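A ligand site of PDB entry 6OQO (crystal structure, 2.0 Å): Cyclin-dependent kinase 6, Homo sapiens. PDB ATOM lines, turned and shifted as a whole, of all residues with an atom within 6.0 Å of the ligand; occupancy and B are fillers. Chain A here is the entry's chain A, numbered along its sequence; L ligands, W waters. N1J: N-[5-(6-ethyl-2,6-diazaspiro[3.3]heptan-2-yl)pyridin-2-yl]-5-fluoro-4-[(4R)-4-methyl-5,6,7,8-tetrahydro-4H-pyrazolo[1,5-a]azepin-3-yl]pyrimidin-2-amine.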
ATOM      1  N   ILE A   9      16.628  25.533 -21.441  1.00  0.00           N
ATOM      2  CA  ILE A   9      16.952  24.698 -22.585  1.00  0.00           C
ATOM      3  C   ILE A   9      17.625  25.513 -23.692  1.00  0.00           C
ATOM      4  O   ILE A   9      18.568  25.038 -24.316  1.00  0.00           O
ATOM      5  CB  ILE A   9      15.686  23.988 -23.100  1.00  0.00           C
ATOM      6  CG1 ILE A   9      14.995  23.240 -21.953  1.00  0.00           C
ATOM      7  CG2 ILE A   9      16.050  23.013 -24.211  1.00  0.00           C
ATOM      8  CD1 ILE A   9      13.748  22.487 -22.395  1.00  0.00           C
ATOM      9  N   GLY A  10      17.146  26.730 -23.924  1.00  0.00           N
ATOM     10  CA  GLY A  10      17.736  27.588 -24.941  1.00  0.00           C
ATOM     11  C   GLY A  10      16.959  28.865 -25.170  1.00  0.00           C
ATOM     12  O   GLY A  10      15.753  28.931 -24.906  1.00  0.00           O
ATOM     13  N   TYR A  14      13.117  32.742 -31.260  1.00  0.00           N
ATOM     14  CA  TYR A  14      11.833  32.074 -30.918  1.00  0.00           C
ATOM     15  C   TYR A  14      11.343  32.525 -29.543  1.00  0.00           C
ATOM     16  O   TYR A  14      10.126  32.546 -29.324  1.00  0.00           O
ATOM     17  CB  TYR A  14      11.997  30.549 -30.980  1.00  0.00           C
ATOM     18  CG  TYR A  14      13.210  30.009 -30.272  1.00  0.00           C
ATOM     19  CD1 TYR A  14      13.228  29.835 -28.900  1.00  0.00           C
ATOM     20  CD2 TYR A  14      14.352  29.658 -30.987  1.00  0.00           C
ATOM     21  CE1 TYR A  14      14.335  29.325 -28.249  1.00  0.00           C
ATOM     22  CE2 TYR A  14      15.465  29.157 -30.348  1.00  0.00           C
ATOM     23  CZ  TYR A  14      15.465  28.984 -28.976  1.00  0.00           C
ATOM     24  OH  TYR A  14      16.562  28.498 -28.343  1.00  0.00           O
ATOM     25  N   VAL A  17      13.128  29.018 -23.901  1.00  0.00           N
ATOM     26  CA  VAL A  17      12.542  27.721 -23.570  1.00  0.00           C
ATOM     27  C   VAL A  17      13.142  27.234 -22.262  1.00  0.00           C
ATOM     28  O   VAL A  17      14.366  27.214 -22.099  1.00  0.00           O
ATOM     29  CB  VAL A  17      12.762  26.707 -24.701  1.00  0.00           C
ATOM     30  CG1 VAL A  17      12.088  25.386 -24.364  1.00  0.00           C
ATOM     31  CG2 VAL A  17      12.245  27.261 -26.021  1.00  0.00           C
ATOM     32  N   ALA A  31       8.083  21.787 -21.292  1.00  0.00           N
ATOM     33  CA  ALA A  31       8.887  22.851 -21.894  1.00  0.00           C
ATOM     34  C   ALA A  31       8.043  24.123 -21.933  1.00  0.00           C
ATOM     35  O   ALA A  31       7.028  24.178 -22.626  1.00  0.00           O
ATOM     36  CB  ALA A  31       9.363  22.466 -23.294  1.00  0.00           C
ATOM     37  N   LYS A  33       7.733  27.990 -22.989  1.00  0.00           N
ATOM     38  CA  LYS A  33       8.249  28.999 -23.910  1.00  0.00           C
ATOM     39  C   LYS A  33       7.560  30.322 -23.615  1.00  0.00           C
ATOM     40  O   LYS A  33       6.361  30.472 -23.876  1.00  0.00           O
ATOM     41  CB  LYS A  33       8.049  28.579 -25.371  1.00  0.00           C
ATOM     42  CG  LYS A  33       8.437  29.663 -26.370  1.00  0.00           C
ATOM     43  CD  LYS A  33       9.074  29.085 -27.618  1.00  0.00           C
ATOM     44  CE  LYS A  33       8.083  28.256 -28.429  1.00  0.00           C
ATOM     45  NZ  LYS A  33       8.699  27.745 -29.680  1.00  0.00           N
ATOM     46  N   VAL A  67       5.389  18.269 -31.723  1.00  0.00           N
ATOM     47  CA  VAL A  67       5.433  18.325 -30.271  1.00  0.00           C
ATOM     48  C   VAL A  67       4.045  18.686 -29.732  1.00  0.00           C
ATOM     49  O   VAL A  67       3.292  19.434 -30.366  1.00  0.00           O
ATOM     50  CB  VAL A  67       6.513  19.314 -29.801  1.00  0.00           C
ATOM     51  CG1 VAL A  67       5.904  20.594 -29.236  1.00  0.00           C
ATOM     52  CG2 VAL A  67       7.438  18.657 -28.782  1.00  0.00           C
ATOM     53  N   PHE A  88       4.713  22.960 -23.709  1.00  0.00           N
ATOM     54  CA  PHE A  88       4.867  21.833 -24.620  1.00  0.00           C
ATOM     55  C   PHE A  88       5.341  20.608 -23.864  1.00  0.00           C
ATOM     56  O   PHE A  88       5.856  20.697 -22.743  1.00  0.00           O
ATOM     57  CB  PHE A  88       5.861  22.165 -25.735  1.00  0.00           C
ATOM     58  CG  PHE A  88       5.443  23.312 -26.617  1.00  0.00           C
ATOM     59  CD1 PHE A  88       4.377  23.178 -27.492  1.00  0.00           C
ATOM     60  CD2 PHE A  88       6.131  24.513 -26.573  1.00  0.00           C
ATOM     61  CE1 PHE A  88       3.993  24.231 -28.297  1.00  0.00           C
ATOM     62  CE2 PHE A  88       5.753  25.575 -27.376  1.00  0.00           C
ATOM     63  CZ  PHE A  88       4.687  25.427 -28.246  1.00  0.00           C
ATOM     64  N   GLU A  89       5.152  19.448 -24.488  1.00  0.00           N
ATOM     65  CA  GLU A  89       5.722  18.223 -23.950  1.00  0.00           C
ATOM     66  C   GLU A  89       7.242  18.288 -24.038  1.00  0.00           C
ATOM     67  O   GLU A  89       7.808  18.942 -24.913  1.00  0.00           O
ATOM     68  CB  GLU A  89       5.202  17.001 -24.710  1.00  0.00           C
ATOM     69  CG  GLU A  89       5.936  16.702 -26.002  1.00  0.00           C
ATOM     70  CD  GLU A  89       5.407  15.462 -26.708  1.00  0.00           C
ATOM     71  OE1 GLU A  89       4.922  15.583 -27.846  1.00  0.00           O
ATOM     72  OE2 GLU A  89       5.487  14.365 -26.106  1.00  0.00           O
ATOM     73  N   HIS A  90       7.910  17.614 -23.100  1.00  0.00           N
ATOM     74  CA  HIS A  90       9.359  17.669 -23.013  1.00  0.00           C
ATOM     75  C   HIS A  90       9.986  16.506 -23.770  1.00  0.00           C
ATOM     76  O   HIS A  90       9.612  15.346 -23.576  1.00  0.00           O
ATOM     77  CB  HIS A  90       9.823  17.647 -21.555  1.00  0.00           C
ATOM     78  CG  HIS A  90      11.310  17.733 -21.396  1.00  0.00           C
ATOM     79  ND1 HIS A  90      12.092  16.636 -21.127  1.00  0.00           N
ATOM     80  CD2 HIS A  90      12.155  18.792 -21.478  1.00  0.00           C
ATOM     81  CE1 HIS A  90      13.360  17.007 -21.041  1.00  0.00           C
ATOM     82  NE2 HIS A  90      13.415  18.311 -21.253  1.00  0.00           N
ATOM     83  N   VAL A  91      10.935  16.833 -24.651  1.00  0.00           N
ATOM     84  CA  VAL A  91      11.755  15.842 -25.347  1.00  0.00           C
ATOM     85  C   VAL A  91      13.179  15.994 -24.862  1.00  0.00           C
ATOM     86  O   VAL A  91      13.667  17.120 -24.654  1.00  0.00           O
ATOM     87  CB  VAL A  91      11.652  16.001 -26.877  1.00  0.00           C
ATOM     88  CG1 VAL A  91      12.334  14.835 -27.575  1.00  0.00           C
ATOM     89  CG2 VAL A  91      10.193  16.105 -27.302  1.00  0.00           C
ATOM     90  N   ASP A  92      13.877  14.867 -24.688  1.00  0.00           N
ATOM     91  CA  ASP A  92      15.167  14.875 -24.013  1.00  0.00           C
ATOM     92  C   ASP A  92      16.291  15.459 -24.867  1.00  0.00           C
ATOM     93  O   ASP A  92      17.238  16.020 -24.309  1.00  0.00           O
ATOM     94  CB  ASP A  92      15.526  13.459 -23.557  1.00  0.00           C
ATOM     95  CG  ASP A  92      14.749  13.028 -22.334  1.00  0.00           C
ATOM     96  OD1 ASP A  92      14.758  13.768 -21.328  1.00  0.00           O
ATOM     97  OD2 ASP A  92      14.122  11.945 -22.375  1.00  0.00           O
ATOM     98  N   GLN A  93      16.215  15.333 -26.182  1.00  0.00           N
ATOM     99  CA  GLN A  93      17.301  15.792 -27.031  1.00  0.00           C
ATOM    100  C   GLN A  93      16.758  16.196 -28.394  1.00  0.00           C
ATOM    101  O   GLN A  93      15.614  15.906 -28.747  1.00  0.00           O
ATOM    102  CB  GLN A  93      18.385  14.725 -27.188  1.00  0.00           C
ATOM    103  CG  GLN A  93      17.927  13.490 -27.933  1.00  0.00           C
ATOM    104  CD  GLN A  93      19.022  12.447 -28.063  1.00  0.00           C
ATOM    105  OE1 GLN A  93      20.035  12.496 -27.372  1.00  0.00           O
ATOM    106  NE2 GLN A  93      18.818  11.488 -28.968  1.00  0.00           N
ATOM    107  N   ASP A  94      17.610  16.880 -29.171  1.00  0.00           N
ATOM    108  CA  ASP A  94      17.304  17.258 -30.534  1.00  0.00           C
ATOM    109  C   ASP A  94      18.081  16.360 -31.503  1.00  0.00           C
ATOM    110  O   ASP A  94      18.639  15.327 -31.103  1.00  0.00           O
ATOM    111  CB  ASP A  94      17.608  18.745 -30.752  1.00  0.00           C
ATOM    112  CG  ASP A  94      19.045  19.101 -30.430  1.00  0.00           C
ATOM    113  OD1 ASP A  94      19.782  18.226 -29.921  1.00  0.00           O
ATOM    114  OD2 ASP A  94      19.438  20.260 -30.689  1.00  0.00           O
ATOM    115  N   THR A  96      20.819  17.211 -33.403  1.00  0.00           N
ATOM    116  CA  THR A  96      22.266  17.383 -33.323  1.00  0.00           C
ATOM    117  C   THR A  96      22.857  16.548 -32.195  1.00  0.00           C
ATOM    118  O   THR A  96      23.903  15.910 -32.377  1.00  0.00           O
ATOM    119  CB  THR A  96      22.616  18.861 -33.137  1.00  0.00           C
ATOM    120  OG1 THR A  96      22.024  19.338 -31.934  1.00  0.00           O
ATOM    121  CG2 THR A  96      22.113  19.680 -34.321  1.00  0.00           C
ATOM    122  N   THR A  97      22.212  16.540 -31.033  1.00  0.00           N
ATOM    123  CA  THR A  97      22.677  15.716 -29.931  1.00  0.00           C
ATOM    124  C   THR A  97      22.612  14.237 -30.276  1.00  0.00           C
ATOM    125  O   THR A  97      23.477  13.462 -29.851  1.00  0.00           O
ATOM    126  CB  THR A  97      21.864  16.006 -28.672  1.00  0.00           C
ATOM    127  OG1 THR A  97      21.856  17.420 -28.414  1.00  0.00           O
ATOM    128  CG2 THR A  97      22.443  15.289 -27.465  1.00  0.00           C
ATOM    129  N   GLN A 139      18.386  21.600 -35.021  1.00  0.00           N
ATOM    130  CA  GLN A 139      18.294  22.151 -33.672  1.00  0.00           C
ATOM    131  C   GLN A 139      16.867  22.163 -33.149  1.00  0.00           C
ATOM    132  O   GLN A 139      16.657  22.094 -31.934  1.00  0.00           O
ATOM    133  CB  GLN A 139      18.885  23.569 -33.644  1.00  0.00           C
ATOM    134  CG  GLN A 139      20.406  23.618 -33.605  1.00  0.00           C
ATOM    135  CD  GLN A 139      21.045  23.219 -34.921  1.00  0.00           C
ATOM    136  OE1 GLN A 139      20.374  23.111 -35.944  1.00  0.00           O
ATOM    137  NE2 GLN A 139      22.354  22.983 -34.886  1.00  0.00           N
ATOM    138  N   ASN A 140      15.872  22.245 -34.038  1.00  0.00           N
ATOM    139  CA  ASN A 140      14.473  22.225 -33.642  1.00  0.00           C
ATOM    140  C   ASN A 140      13.758  20.950 -34.068  1.00  0.00           C
ATOM    141  O   ASN A 140      12.517  20.924 -34.132  1.00  0.00           O
ATOM    142  CB  ASN A 140      13.748  23.465 -34.177  1.00  0.00           C
ATOM    143  CG  ASN A 140      13.921  23.648 -35.668  1.00  0.00           C
ATOM    144  OD1 ASN A 140      13.804  22.699 -36.451  1.00  0.00           O
ATOM    145  ND2 ASN A 140      14.185  24.877 -36.085  1.00  0.00           N
ATOM    146  N   LEU A 142      13.247  17.362 -32.668  1.00  0.00           N
ATOM    147  CA  LEU A 142      13.432  16.652 -31.407  1.00  0.00           C
ATOM    148  C   LEU A 142      13.319  15.151 -31.608  1.00  0.00           C
ATOM    149  O   LEU A 142      12.524  14.672 -32.425  1.00  0.00           O
ATOM    150  CB  LEU A 142      12.403  17.131 -30.383  1.00  0.00           C
ATOM    151  CG  LEU A 142      12.316  18.654 -30.232  1.00  0.00           C
ATOM    152  CD1 LEU A 142      11.267  19.045 -29.203  1.00  0.00           C
ATOM    153  CD2 LEU A 142      13.672  19.243 -29.879  1.00  0.00           C
ATOM    154  N   ALA A 152       9.305  21.046 -33.696  1.00  0.00           N
ATOM    155  CA  ALA A 152       9.087  22.088 -32.696  1.00  0.00           C
ATOM    156  C   ALA A 152       9.494  23.426 -33.295  1.00  0.00           C
ATOM    157  O   ALA A 152      10.120  23.502 -34.352  1.00  0.00           O
ATOM    158  CB  ALA A 152       9.861  21.804 -31.408  1.00  0.00           C
ATOM    159  N   ASP A 153       9.121  24.494 -32.578  1.00  0.00           N
ATOM    160  CA  ASP A 153       9.468  25.865 -32.944  1.00  0.00           C
ATOM    161  C   ASP A 153       8.931  26.221 -34.337  1.00  0.00           C
ATOM    162  O   ASP A 153       9.684  26.422 -35.300  1.00  0.00           O
ATOM    163  CB  ASP A 153      10.980  26.089 -32.859  1.00  0.00           C
ATOM    164  CG  ASP A 153      11.357  27.558 -32.904  1.00  0.00           C
ATOM    165  OD1 ASP A 153      10.452  28.410 -32.907  1.00  0.00           O
ATOM    166  OD2 ASP A 153      12.575  27.852 -32.935  1.00  0.00           O
HETATM  167  C4  N1J L   1      21.583  22.557 -25.222  1.00  0.00           C
HETATM  168  C5  N1J L   1      20.786  21.450 -25.901  1.00  0.00           C
HETATM  169  C6  N1J L   1      22.108  20.971 -26.486  1.00  0.00           C
HETATM  170  C11 N1J L   1      16.830  20.654 -27.130  1.00  0.00           C
HETATM  171  C7  N1J L   1      19.879  20.512 -25.109  1.00  0.00           C
HETATM  172  C9  N1J L   1      19.565  21.738 -26.771  1.00  0.00           C
HETATM  173  C10 N1J L   1      17.760  20.261 -26.171  1.00  0.00           C
HETATM  174  C12 N1J L   1      15.479  20.522 -26.852  1.00  0.00           C
HETATM  175  C13 N1J L   1      15.092  20.009 -25.619  1.00  0.00           C
HETATM  176  N3  N1J L   1      22.747  22.228 -26.060  1.00  0.00           N
HETATM  177  C1  N1J L   1      24.994  21.211 -26.051  1.00  0.00           C
HETATM  178  C15 N1J L   1      17.306  19.756 -24.968  1.00  0.00           C
HETATM  179  C17 N1J L   1      12.609  20.438 -25.790  1.00  0.00           C
HETATM  180  C19 N1J L   1      10.331  20.325 -25.999  1.00  0.00           C
HETATM  181  C2  N1J L   1      23.936  21.962 -25.238  1.00  0.00           C
HETATM  182  C20 N1J L   1      10.336  21.482 -26.759  1.00  0.00           C
HETATM  183  C21 N1J L   1      11.569  22.121 -27.022  1.00  0.00           C
HETATM  184  C23 N1J L   1      11.625  23.377 -27.833  1.00  0.00           C
HETATM  185  C24 N1J L   1      10.497  24.118 -28.241  1.00  0.00           C
HETATM  186  C27 N1J L   1      12.730  24.048 -28.319  1.00  0.00           C
HETATM  187  C28 N1J L   1      14.190  23.653 -28.141  1.00  0.00           C
HETATM  188  C29 N1J L   1      14.887  23.551 -29.501  1.00  0.00           C
HETATM  189  C30 N1J L   1      15.197  24.943 -30.066  1.00  0.00           C
HETATM  190  C31 N1J L   1      13.966  25.505 -30.757  1.00  0.00           C
HETATM  191  C32 N1J L   1      13.079  26.159 -29.687  1.00  0.00           C
HETATM  192  C33 N1J L   1      14.927  24.638 -27.220  1.00  0.00           C
HETATM  193  F34 N1J L   1       9.149  21.946 -27.214  1.00  0.00           F
HETATM  194  N14 N1J L   1      16.009  19.643 -24.735  1.00  0.00           N
HETATM  195  N16 N1J L   1      13.753  19.835 -25.247  1.00  0.00           N
HETATM  196  N18 N1J L   1      11.464  19.837 -25.537  1.00  0.00           N
HETATM  197  N22 N1J L   1      12.668  21.556 -26.504  1.00  0.00           N
HETATM  198  N25 N1J L   1      10.888  25.156 -28.925  1.00  0.00           N
HETATM  199  N26 N1J L   1      12.284  25.134 -28.999  1.00  0.00           N
HETATM  200  N8  N1J L   1      19.149  20.366 -26.394  1.00  0.00           N
HETATM  201  O   HOH W   1      19.846  18.203 -27.360  1.00  0.00           O
HETATM  202  O   HOH W   2      16.020  19.115 -21.844  1.00  0.00           O
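The backbone carbonyl oxygen (O) of Val 91 sits close to a nitrogen (N16) of the ligand (2.8 Å). The side-chain amino group (NZ) of Lys 33 lies within hydrogen-bond range of a nitrogen (N25) of the ligand. The backbone NH (N) of Val 91 sits at hydrogen-bond distance from a nitrogen (N18) of the ligand (3.2 Å).
Water W1 lies within hydrogen-bond range of the side-chain hydroxyl of Thr 97 and the side-chain carboxylate of Asp 94. Water W2 lies within hydrogen-bond range of a ring nitrogen (NE2) of His 90 and a nitrogen (N14) of the ligand.
The backbone carbonyl oxygen (O) of Ala 31 is in hydrogen-bond range of the backbone NH (N) of Phe 88, at 2.8 Å. The backbone NH (N) of Ala 152 is in hydrogen-bond range of the backbone carbonyl oxygen (O) of Asn 140 (3.2 Å). The backbone carbonyl oxygen (O) of Gly 10 is in hydrogen-bond range of the backbone NH (N) of Val 17, at 2.8 Å. The side-chain carboxylate (OD1) of Asp 153 is in salt-bridge range of the side-chain amino group (NZ) of Lys 33, 3.7 Å away. The backbone NH (N) of Ile 9 lies within hydrogen-bond range of the backbone carbonyl oxygen (O) of Val 17 (2.9 Å).
Ile 9 touches the ligand. Tyr 14 touches the ligand. Val 17 touches the ligand. CB of Ala 31 touches C19 of the ligand (3.6 Å). CB of Phe 88 touches F34 of the ligand (3.6 Å). Glu 89 touches the ligand (O to C19, 3.1 Å). His 90 touches the ligand (CA to N18, 3.9 Å). O of Asp 92 touches C15 of the ligand (3.8 Å). Gln 139 touches the ligand (O to C29, 3.3 Å). Asn 140 touches the ligand. Leu 142 touches the ligand. Ala 152 touches the ligand. OD2 of Asp 153 touches C31 of the ligand, at 3.5 Å. Hydrophobic or aromatic side chains within 4 Å of the ligand: Ile 9, Tyr 14, Val 17, Ala 31, Phe 88, Leu 142 and Ala 152. Along chain A the residues within 4 Å of the ligand span positions 9 to 153. The nearest printed residue that does not touch the ligand is Val 67 (4.03 Å).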
